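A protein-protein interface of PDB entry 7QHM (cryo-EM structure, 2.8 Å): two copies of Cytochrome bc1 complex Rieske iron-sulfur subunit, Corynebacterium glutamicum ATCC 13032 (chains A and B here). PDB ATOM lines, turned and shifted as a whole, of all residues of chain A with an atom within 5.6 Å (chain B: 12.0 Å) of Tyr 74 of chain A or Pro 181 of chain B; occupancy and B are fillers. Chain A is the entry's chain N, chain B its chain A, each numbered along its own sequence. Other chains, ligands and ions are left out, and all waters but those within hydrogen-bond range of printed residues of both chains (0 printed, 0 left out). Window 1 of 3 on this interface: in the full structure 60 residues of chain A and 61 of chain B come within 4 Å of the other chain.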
ATOM      1  N   GLY A  69       8.597 -17.321  24.937  1.00  0.00           N
ATOM      2  CA  GLY A  69       9.386 -18.378  25.534  1.00  0.00           C
ATOM      3  C   GLY A  69      10.248 -19.093  24.519  1.00  0.00           C
ATOM      4  O   GLY A  69      11.373 -19.490  24.824  1.00  0.00           O
ATOM      5  N   PHE A  70       9.735 -19.276  23.299  1.00  0.00           N
ATOM      6  CA  PHE A  70      10.531 -19.943  22.275  1.00  0.00           C
ATOM      7  C   PHE A  70      11.773 -19.135  21.951  1.00  0.00           C
ATOM      8  O   PHE A  70      12.884 -19.670  21.918  1.00  0.00           O
ATOM      9  CB  PHE A  70       9.727 -20.179  20.995  1.00  0.00           C
ATOM     10  CG  PHE A  70      10.530 -20.859  19.918  1.00  0.00           C
ATOM     11  CD1 PHE A  70      10.669 -22.233  19.910  1.00  0.00           C
ATOM     12  CD2 PHE A  70      11.183 -20.131  18.944  1.00  0.00           C
ATOM     13  CE1 PHE A  70      11.427 -22.858  18.946  1.00  0.00           C
ATOM     14  CE2 PHE A  70      11.937 -20.757  17.991  1.00  0.00           C
ATOM     15  CZ  PHE A  70      12.056 -22.121  17.990  1.00  0.00           C
ATOM     16  N   LEU A  71      11.597 -17.847  21.668  1.00  0.00           N
ATOM     17  CA  LEU A  71      12.735 -17.027  21.286  1.00  0.00           C
ATOM     18  C   LEU A  71      13.720 -16.910  22.433  1.00  0.00           C
ATOM     19  O   LEU A  71      14.936 -16.959  22.224  1.00  0.00           O
ATOM     20  CB  LEU A  71      12.258 -15.649  20.838  1.00  0.00           C
ATOM     21  CG  LEU A  71      11.320 -15.614  19.630  1.00  0.00           C
ATOM     22  CD1 LEU A  71      10.867 -14.194  19.379  1.00  0.00           C
ATOM     23  CD2 LEU A  71      11.971 -16.183  18.381  1.00  0.00           C
ATOM     24  N   ALA A  72      13.215 -16.773  23.657  1.00  0.00           N
ATOM     25  CA  ALA A  72      14.093 -16.740  24.818  1.00  0.00           C
ATOM     26  C   ALA A  72      14.893 -18.026  24.928  1.00  0.00           C
ATOM     27  O   ALA A  72      16.107 -17.997  25.140  1.00  0.00           O
ATOM     28  CB  ALA A  72      13.273 -16.509  26.084  1.00  0.00           C
ATOM     29  N   THR A  73      14.227 -19.170  24.781  1.00  0.00           N
ATOM     30  CA  THR A  73      14.922 -20.450  24.852  1.00  0.00           C
ATOM     31  C   THR A  73      15.922 -20.593  23.716  1.00  0.00           C
ATOM     32  O   THR A  73      17.083 -20.945  23.939  1.00  0.00           O
ATOM     33  CB  THR A  73      13.904 -21.587  24.818  1.00  0.00           C
ATOM     34  OG1 THR A  73      12.939 -21.378  25.851  1.00  0.00           O
ATOM     35  CG2 THR A  73      14.562 -22.952  25.014  1.00  0.00           C
ATOM     36  N   TYR A  74      15.490 -20.326  22.486  1.00  0.00           N
ATOM     37  CA  TYR A  74      16.359 -20.523  21.337  1.00  0.00           C
ATOM     38  C   TYR A  74      17.594 -19.643  21.386  1.00  0.00           C
ATOM     39  O   TYR A  74      18.606 -19.991  20.774  1.00  0.00           O
ATOM     40  CB  TYR A  74      15.591 -20.262  20.045  1.00  0.00           C
ATOM     41  CG  TYR A  74      16.373 -20.611  18.804  1.00  0.00           C
ATOM     42  CD1 TYR A  74      16.476 -21.916  18.377  1.00  0.00           C
ATOM     43  CD2 TYR A  74      17.013 -19.634  18.068  1.00  0.00           C
ATOM     44  CE1 TYR A  74      17.189 -22.236  17.257  1.00  0.00           C
ATOM     45  CE2 TYR A  74      17.727 -19.943  16.950  1.00  0.00           C
ATOM     46  CZ  TYR A  74      17.817 -21.245  16.547  1.00  0.00           C
ATOM     47  OH  TYR A  74      18.537 -21.560  15.423  1.00  0.00           O
ATOM     48  N   ILE A  75      17.548 -18.522  22.098  1.00  0.00           N
ATOM     49  CA  ILE A  75      18.695 -17.629  22.194  1.00  0.00           C
ATOM     50  C   ILE A  75      19.517 -17.998  23.422  1.00  0.00           C
ATOM     51  O   ILE A  75      20.687 -18.370  23.308  1.00  0.00           O
ATOM     52  CB  ILE A  75      18.255 -16.151  22.238  1.00  0.00           C
ATOM     53  CG1 ILE A  75      17.509 -15.762  20.957  1.00  0.00           C
ATOM     54  CG2 ILE A  75      19.470 -15.238  22.402  1.00  0.00           C
ATOM     55  CD1 ILE A  75      16.656 -14.519  21.082  1.00  0.00           C
ATOM     56  N   PHE A  76      18.903 -17.919  24.601  1.00  0.00           N
ATOM     57  CA  PHE A  76      19.633 -17.833  25.857  1.00  0.00           C
ATOM     58  C   PHE A  76      19.769 -19.147  26.606  1.00  0.00           C
ATOM     59  O   PHE A  76      20.582 -19.223  27.530  1.00  0.00           O
ATOM     60  CB  PHE A  76      18.954 -16.828  26.780  1.00  0.00           C
ATOM     61  CG  PHE A  76      18.813 -15.475  26.186  1.00  0.00           C
ATOM     62  CD1 PHE A  76      19.893 -14.626  26.123  1.00  0.00           C
ATOM     63  CD2 PHE A  76      17.594 -15.045  25.692  1.00  0.00           C
ATOM     64  CE1 PHE A  76      19.769 -13.384  25.578  1.00  0.00           C
ATOM     65  CE2 PHE A  76      17.463 -13.799  25.150  1.00  0.00           C
ATOM     66  CZ  PHE A  76      18.552 -12.966  25.091  1.00  0.00           C
ATOM     67  N   TRP A  77      18.994 -20.161  26.271  1.00  0.00           N
ATOM     68  CA  TRP A  77      19.199 -21.458  26.889  1.00  0.00           C
ATOM     69  C   TRP A  77      20.521 -22.047  26.392  1.00  0.00           C
ATOM     70  O   TRP A  77      20.815 -21.957  25.199  1.00  0.00           O
ATOM     71  CB  TRP A  77      18.047 -22.387  26.542  1.00  0.00           C
ATOM     72  CG  TRP A  77      17.923 -23.580  27.402  1.00  0.00           C
ATOM     73  CD1 TRP A  77      18.694 -24.690  27.372  1.00  0.00           C
ATOM     74  CD2 TRP A  77      16.941 -23.799  28.409  1.00  0.00           C
ATOM     75  NE1 TRP A  77      18.264 -25.589  28.304  1.00  0.00           N
ATOM     76  CE2 TRP A  77      17.185 -25.063  28.958  1.00  0.00           C
ATOM     77  CE3 TRP A  77      15.880 -23.042  28.908  1.00  0.00           C
ATOM     78  CZ2 TRP A  77      16.412 -25.591  29.977  1.00  0.00           C
ATOM     79  CZ3 TRP A  77      15.119 -23.565  29.917  1.00  0.00           C
ATOM     80  CH2 TRP A  77      15.384 -24.830  30.442  1.00  0.00           C
ATOM     81  N   TYR A  95      17.233 -28.793  26.146  1.00  0.00           N
ATOM     82  CA  TYR A  95      17.162 -27.718  25.166  1.00  0.00           C
ATOM     83  C   TYR A  95      16.102 -27.998  24.110  1.00  0.00           C
ATOM     84  O   TYR A  95      15.122 -27.260  24.007  1.00  0.00           O
ATOM     85  CB  TYR A  95      18.525 -27.511  24.509  1.00  0.00           C
ATOM     86  CG  TYR A  95      18.554 -26.406  23.492  1.00  0.00           C
ATOM     87  CD1 TYR A  95      18.365 -25.096  23.869  1.00  0.00           C
ATOM     88  CD2 TYR A  95      18.775 -26.673  22.158  1.00  0.00           C
ATOM     89  CE1 TYR A  95      18.390 -24.086  22.953  1.00  0.00           C
ATOM     90  CE2 TYR A  95      18.801 -25.668  21.232  1.00  0.00           C
ATOM     91  CZ  TYR A  95      18.610 -24.375  21.638  1.00  0.00           C
ATOM     92  OH  TYR A  95      18.636 -23.354  20.727  1.00  0.00           O
ATOM     93  N   LEU A  99      12.466 -26.332  23.291  1.00  0.00           N
ATOM     94  CA  LEU A  99      12.175 -25.708  22.004  1.00  0.00           C
ATOM     95  C   LEU A  99      10.809 -26.136  21.499  1.00  0.00           C
ATOM     96  O   LEU A  99       9.992 -25.303  21.097  1.00  0.00           O
ATOM     97  CB  LEU A  99      13.233 -26.059  20.957  1.00  0.00           C
ATOM     98  CG  LEU A  99      14.615 -25.414  20.984  1.00  0.00           C
ATOM     99  CD1 LEU A  99      15.381 -25.866  19.779  1.00  0.00           C
ATOM    100  CD2 LEU A  99      14.573 -23.910  21.011  1.00  0.00           C
ATOM    101  N   VAL B 172       2.426 -12.685  14.043  1.00  0.00           N
ATOM    102  CA  VAL B 172       3.801 -12.310  13.740  1.00  0.00           C
ATOM    103  C   VAL B 172       4.772 -13.075  14.623  1.00  0.00           C
ATOM    104  O   VAL B 172       5.861 -13.450  14.177  1.00  0.00           O
ATOM    105  CB  VAL B 172       4.003 -10.787  13.865  1.00  0.00           C
ATOM    106  CG1 VAL B 172       3.105 -10.050  12.881  1.00  0.00           C
ATOM    107  CG2 VAL B 172       3.768 -10.299  15.279  1.00  0.00           C
ATOM    108  N   LEU B 173       4.403 -13.349  15.872  1.00  0.00           N
ATOM    109  CA  LEU B 173       5.307 -14.075  16.749  1.00  0.00           C
ATOM    110  C   LEU B 173       5.420 -15.538  16.346  1.00  0.00           C
ATOM    111  O   LEU B 173       6.496 -16.126  16.458  1.00  0.00           O
ATOM    112  CB  LEU B 173       4.826 -13.936  18.186  1.00  0.00           C
ATOM    113  CG  LEU B 173       5.743 -14.406  19.308  1.00  0.00           C
ATOM    114  CD1 LEU B 173       7.020 -13.602  19.377  1.00  0.00           C
ATOM    115  CD2 LEU B 173       4.987 -14.324  20.624  1.00  0.00           C
ATOM    116  N   ALA B 174       4.338 -16.138  15.857  1.00  0.00           N
ATOM    117  CA  ALA B 174       4.437 -17.479  15.300  1.00  0.00           C
ATOM    118  C   ALA B 174       5.298 -17.477  14.050  1.00  0.00           C
ATOM    119  O   ALA B 174       6.057 -18.419  13.820  1.00  0.00           O
ATOM    120  CB  ALA B 174       3.046 -18.029  14.990  1.00  0.00           C
ATOM    121  N   GLY B 175       5.189 -16.438  13.223  1.00  0.00           N
ATOM    122  CA  GLY B 175       6.083 -16.331  12.083  1.00  0.00           C
ATOM    123  C   GLY B 175       7.538 -16.288  12.504  1.00  0.00           C
ATOM    124  O   GLY B 175       8.392 -16.954  11.906  1.00  0.00           O
ATOM    125  N   LEU B 176       7.834 -15.521  13.558  1.00  0.00           N
ATOM    126  CA  LEU B 176       9.184 -15.499  14.108  1.00  0.00           C
ATOM    127  C   LEU B 176       9.590 -16.875  14.613  1.00  0.00           C
ATOM    128  O   LEU B 176      10.729 -17.307  14.416  1.00  0.00           O
ATOM    129  CB  LEU B 176       9.280 -14.474  15.233  1.00  0.00           C
ATOM    130  CG  LEU B 176       9.084 -13.013  14.854  1.00  0.00           C
ATOM    131  CD1 LEU B 176       8.999 -12.172  16.109  1.00  0.00           C
ATOM    132  CD2 LEU B 176      10.206 -12.527  13.961  1.00  0.00           C
ATOM    133  N   THR B 177       8.667 -17.577  15.266  1.00  0.00           N
ATOM    134  CA  THR B 177       8.966 -18.912  15.764  1.00  0.00           C
ATOM    135  C   THR B 177       9.264 -19.870  14.622  1.00  0.00           C
ATOM    136  O   THR B 177      10.099 -20.765  14.769  1.00  0.00           O
ATOM    137  CB  THR B 177       7.797 -19.422  16.612  1.00  0.00           C
ATOM    138  OG1 THR B 177       7.638 -18.579  17.758  1.00  0.00           O
ATOM    139  CG2 THR B 177       8.020 -20.841  17.078  1.00  0.00           C
ATOM    140  N   ILE B 178       8.598 -19.698  13.482  1.00  0.00           N
ATOM    141  CA  ILE B 178       8.874 -20.544  12.326  1.00  0.00           C
ATOM    142  C   ILE B 178      10.267 -20.253  11.787  1.00  0.00           C
ATOM    143  O   ILE B 178      11.052 -21.171  11.533  1.00  0.00           O
ATOM    144  CB  ILE B 178       7.809 -20.351  11.227  1.00  0.00           C
ATOM    145  CG1 ILE B 178       6.415 -20.805  11.674  1.00  0.00           C
ATOM    146  CG2 ILE B 178       8.204 -21.089   9.945  1.00  0.00           C
ATOM    147  CD1 ILE B 178       6.227 -22.267  11.866  1.00  0.00           C
ATOM    148  N   ILE B 179      10.595 -18.970  11.594  1.00  0.00           N
ATOM    149  CA  ILE B 179      11.840 -18.614  10.911  1.00  0.00           C
ATOM    150  C   ILE B 179      13.042 -18.478  11.837  1.00  0.00           C
ATOM    151  O   ILE B 179      14.166 -18.300  11.345  1.00  0.00           O
ATOM    152  CB  ILE B 179      11.684 -17.304  10.113  1.00  0.00           C
ATOM    153  CG1 ILE B 179      11.450 -16.103  11.045  1.00  0.00           C
ATOM    154  CG2 ILE B 179      10.566 -17.468   9.093  1.00  0.00           C
ATOM    155  CD1 ILE B 179      11.161 -14.798  10.333  1.00  0.00           C
ATOM    156  N   ALA B 180      12.852 -18.547  13.152  1.00  0.00           N
ATOM    157  CA  ALA B 180      13.975 -18.369  14.067  1.00  0.00           C
ATOM    158  C   ALA B 180      15.062 -19.425  13.917  1.00  0.00           C
ATOM    159  O   ALA B 180      16.243 -19.072  14.068  1.00  0.00           O
ATOM    160  CB  ALA B 180      13.463 -18.331  15.508  1.00  0.00           C
ATOM    161  N   PRO B 181      14.767 -20.700  13.637  1.00  0.00           N
ATOM    162  CA  PRO B 181      15.848 -21.669  13.406  1.00  0.00           C
ATOM    163  C   PRO B 181      16.781 -21.338  12.247  1.00  0.00           C
ATOM    164  O   PRO B 181      17.824 -21.991  12.127  1.00  0.00           O
ATOM    165  CB  PRO B 181      15.085 -22.973  13.163  1.00  0.00           C
ATOM    166  CG  PRO B 181      13.896 -22.830  13.985  1.00  0.00           C
ATOM    167  CD  PRO B 181      13.499 -21.395  13.912  1.00  0.00           C
ATOM    168  N   MET B 182      16.486 -20.334  11.422  1.00  0.00           N
ATOM    169  CA  MET B 182      17.473 -19.857  10.460  1.00  0.00           C
ATOM    170  C   MET B 182      18.707 -19.281  11.136  1.00  0.00           C
ATOM    171  O   MET B 182      19.737 -19.120  10.477  1.00  0.00           O
ATOM    172  CB  MET B 182      16.867 -18.789   9.550  1.00  0.00           C
ATOM    173  CG  MET B 182      15.745 -19.281   8.670  1.00  0.00           C
ATOM    174  SD  MET B 182      16.213 -20.610   7.532  1.00  0.00           S
ATOM    175  CE  MET B 182      17.297 -19.743   6.405  1.00  0.00           C
ATOM    176  N   GLY B 183      18.636 -18.967  12.426  1.00  0.00           N
ATOM    177  CA  GLY B 183      19.814 -18.609  13.174  1.00  0.00           C
ATOM    178  C   GLY B 183      20.788 -19.741  13.411  1.00  0.00           C
ATOM    179  O   GLY B 183      21.813 -19.519  14.059  1.00  0.00           O
ATOM    180  N   GLY B 184      20.490 -20.954  12.944  1.00  0.00           N
ATOM    181  CA  GLY B 184      21.512 -21.980  12.885  1.00  0.00           C
ATOM    182  C   GLY B 184      22.552 -21.746  11.816  1.00  0.00           C
ATOM    183  O   GLY B 184      23.601 -22.395  11.843  1.00  0.00           O
ATOM    184  N   MET B 185      22.283 -20.839  10.880  1.00  0.00           N
ATOM    185  CA  MET B 185      23.254 -20.441   9.875  1.00  0.00           C
ATOM    186  C   MET B 185      24.110 -19.269  10.327  1.00  0.00           C
ATOM    187  O   MET B 185      25.253 -19.138   9.874  1.00  0.00           O
ATOM    188  CB  MET B 185      22.540 -20.054   8.581  1.00  0.00           C
ATOM    189  CG  MET B 185      21.584 -21.097   8.037  1.00  0.00           C
ATOM    190  SD  MET B 185      20.725 -20.552   6.550  1.00  0.00           S
ATOM    191  CE  MET B 185      22.074 -20.395   5.378  1.00  0.00           C
ATOM    192  N   ILE B 186      23.582 -18.409  11.199  1.00  0.00           N
ATOM    193  CA  ILE B 186      24.335 -17.247  11.648  1.00  0.00           C
ATOM    194  C   ILE B 186      25.572 -17.708  12.406  1.00  0.00           C
ATOM    195  O   ILE B 186      25.515 -18.622  13.237  1.00  0.00           O
ATOM    196  CB  ILE B 186      23.448 -16.329  12.506  1.00  0.00           C
ATOM    197  CG1 ILE B 186      22.346 -15.713  11.646  1.00  0.00           C
ATOM    198  CG2 ILE B 186      24.278 -15.216  13.164  1.00  0.00           C
ATOM    199  CD1 ILE B 186      21.217 -15.077  12.416  1.00  0.00           C
ATOM    200  N   LYS B 187      26.702 -17.074  12.105  1.00  0.00           N
ATOM    201  CA  LYS B 187      27.976 -17.391  12.737  1.00  0.00           C
ATOM    202  C   LYS B 187      28.774 -16.107  12.886  1.00  0.00           C
ATOM    203  O   LYS B 187      29.006 -15.399  11.903  1.00  0.00           O
ATOM    204  CB  LYS B 187      28.765 -18.412  11.920  1.00  0.00           C
ATOM    205  CG  LYS B 187      28.214 -19.814  11.980  1.00  0.00           C
ATOM    206  CD  LYS B 187      28.968 -20.768  11.075  1.00  0.00           C
ATOM    207  CE  LYS B 187      30.383 -21.001  11.546  1.00  0.00           C
ATOM    208  NZ  LYS B 187      31.015 -22.163  10.871  1.00  0.00           N
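The side-chain hydroxyl (OH) of Tyr 74 of chain A sits at hydrogen-bond distance from the backbone NH (N) of Gly 184 of chain B (3.2 Å).
The side-chain hydroxyl (OH) of Tyr 74 of chain A sits close to the backbone carbonyl oxygen (O) of Pro 181 of chain B, 3.4 Å away.
No position is printed for both chains.
Phe 70 of chain A touches two residues of chain B.
Leu 71 of chain A touches just these residues of chain B: Leu 173 and Ala 180.
No residue of chain B comes within 4 Å of Thr 73 of chain A.
No residue of chain B comes within 4 Å of Ile 75 of chain A.
No residue of chain B comes within 4 Å of Phe 76 of chain A.
Tyr 95 of chain A touches none of the printed residues of chain B.
Printed residues of chain A within 4 Å of Leu 173 of chain B: Leu 71 (3.9 Å).
Printed residues of chain A within 4 Å of Thr 177 of chain B: Phe 70 (3.7 Å).
Of the printed residues of chain A, Ala 180 of chain B touches Phe 70 (3.8 Å), Leu 71 (3.9 Å) and Tyr 74 (3.4 Å).
Of the printed residues of chain A, Pro 181 of chain B touches Tyr 74 (3.4 Å).
Printed residues of chain A within 4 Å of Gly 183 of chain B: Tyr 74.
Printed residues of chain A within 4 Å of Gly 184 of chain B: Tyr 74 (3.2 Å).
The nearest residue of chain A that does not touch Pro 181 of chain B is Phe 70 of chain A (4.4 Å).
The nearest printed residue of chain A that does not touch Thr 177 of chain B is Leu 71 of chain A (4.8 Å).
Among the printed residues, merely in contact across the chains: Phe 70 of chain A with Thr 177 of chain B, Phe 70 of chain A with Ala 180 of chain B, Leu 71 of chain A with Leu 173 of chain B, Leu 71 of chain A with Ala 180 of chain B, Tyr 74 of chain A with Ala 180 of chain B and Tyr 74 of chain A with Gly 183 of chain B.
Of the 11 printed residues of chain A, 3 touch a printed residue of chain B.
Hydrophobic or aromatic side chains of chain A that line the printed part of chain B: Phe 70, Leu 71 and Tyr 74.
Among the printed residues, 8 pairs touch across the chains.
Among the printed residues, no Asp or Glu carboxylate lies within 4 Å of a Lys or Arg side-chain nitrogen of the other chain.
The backbone carbonyl oxygen (O) of Tyr 74 of chain A sits at hydrogen-bond distance from the side-chain hydroxyl (OH) of Tyr 95 of chain A (3.4 Å).
OG1 of Thr 177 of chain B lies within hydrogen-bond range of O of Leu 173 of chain B (3.0 Å).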
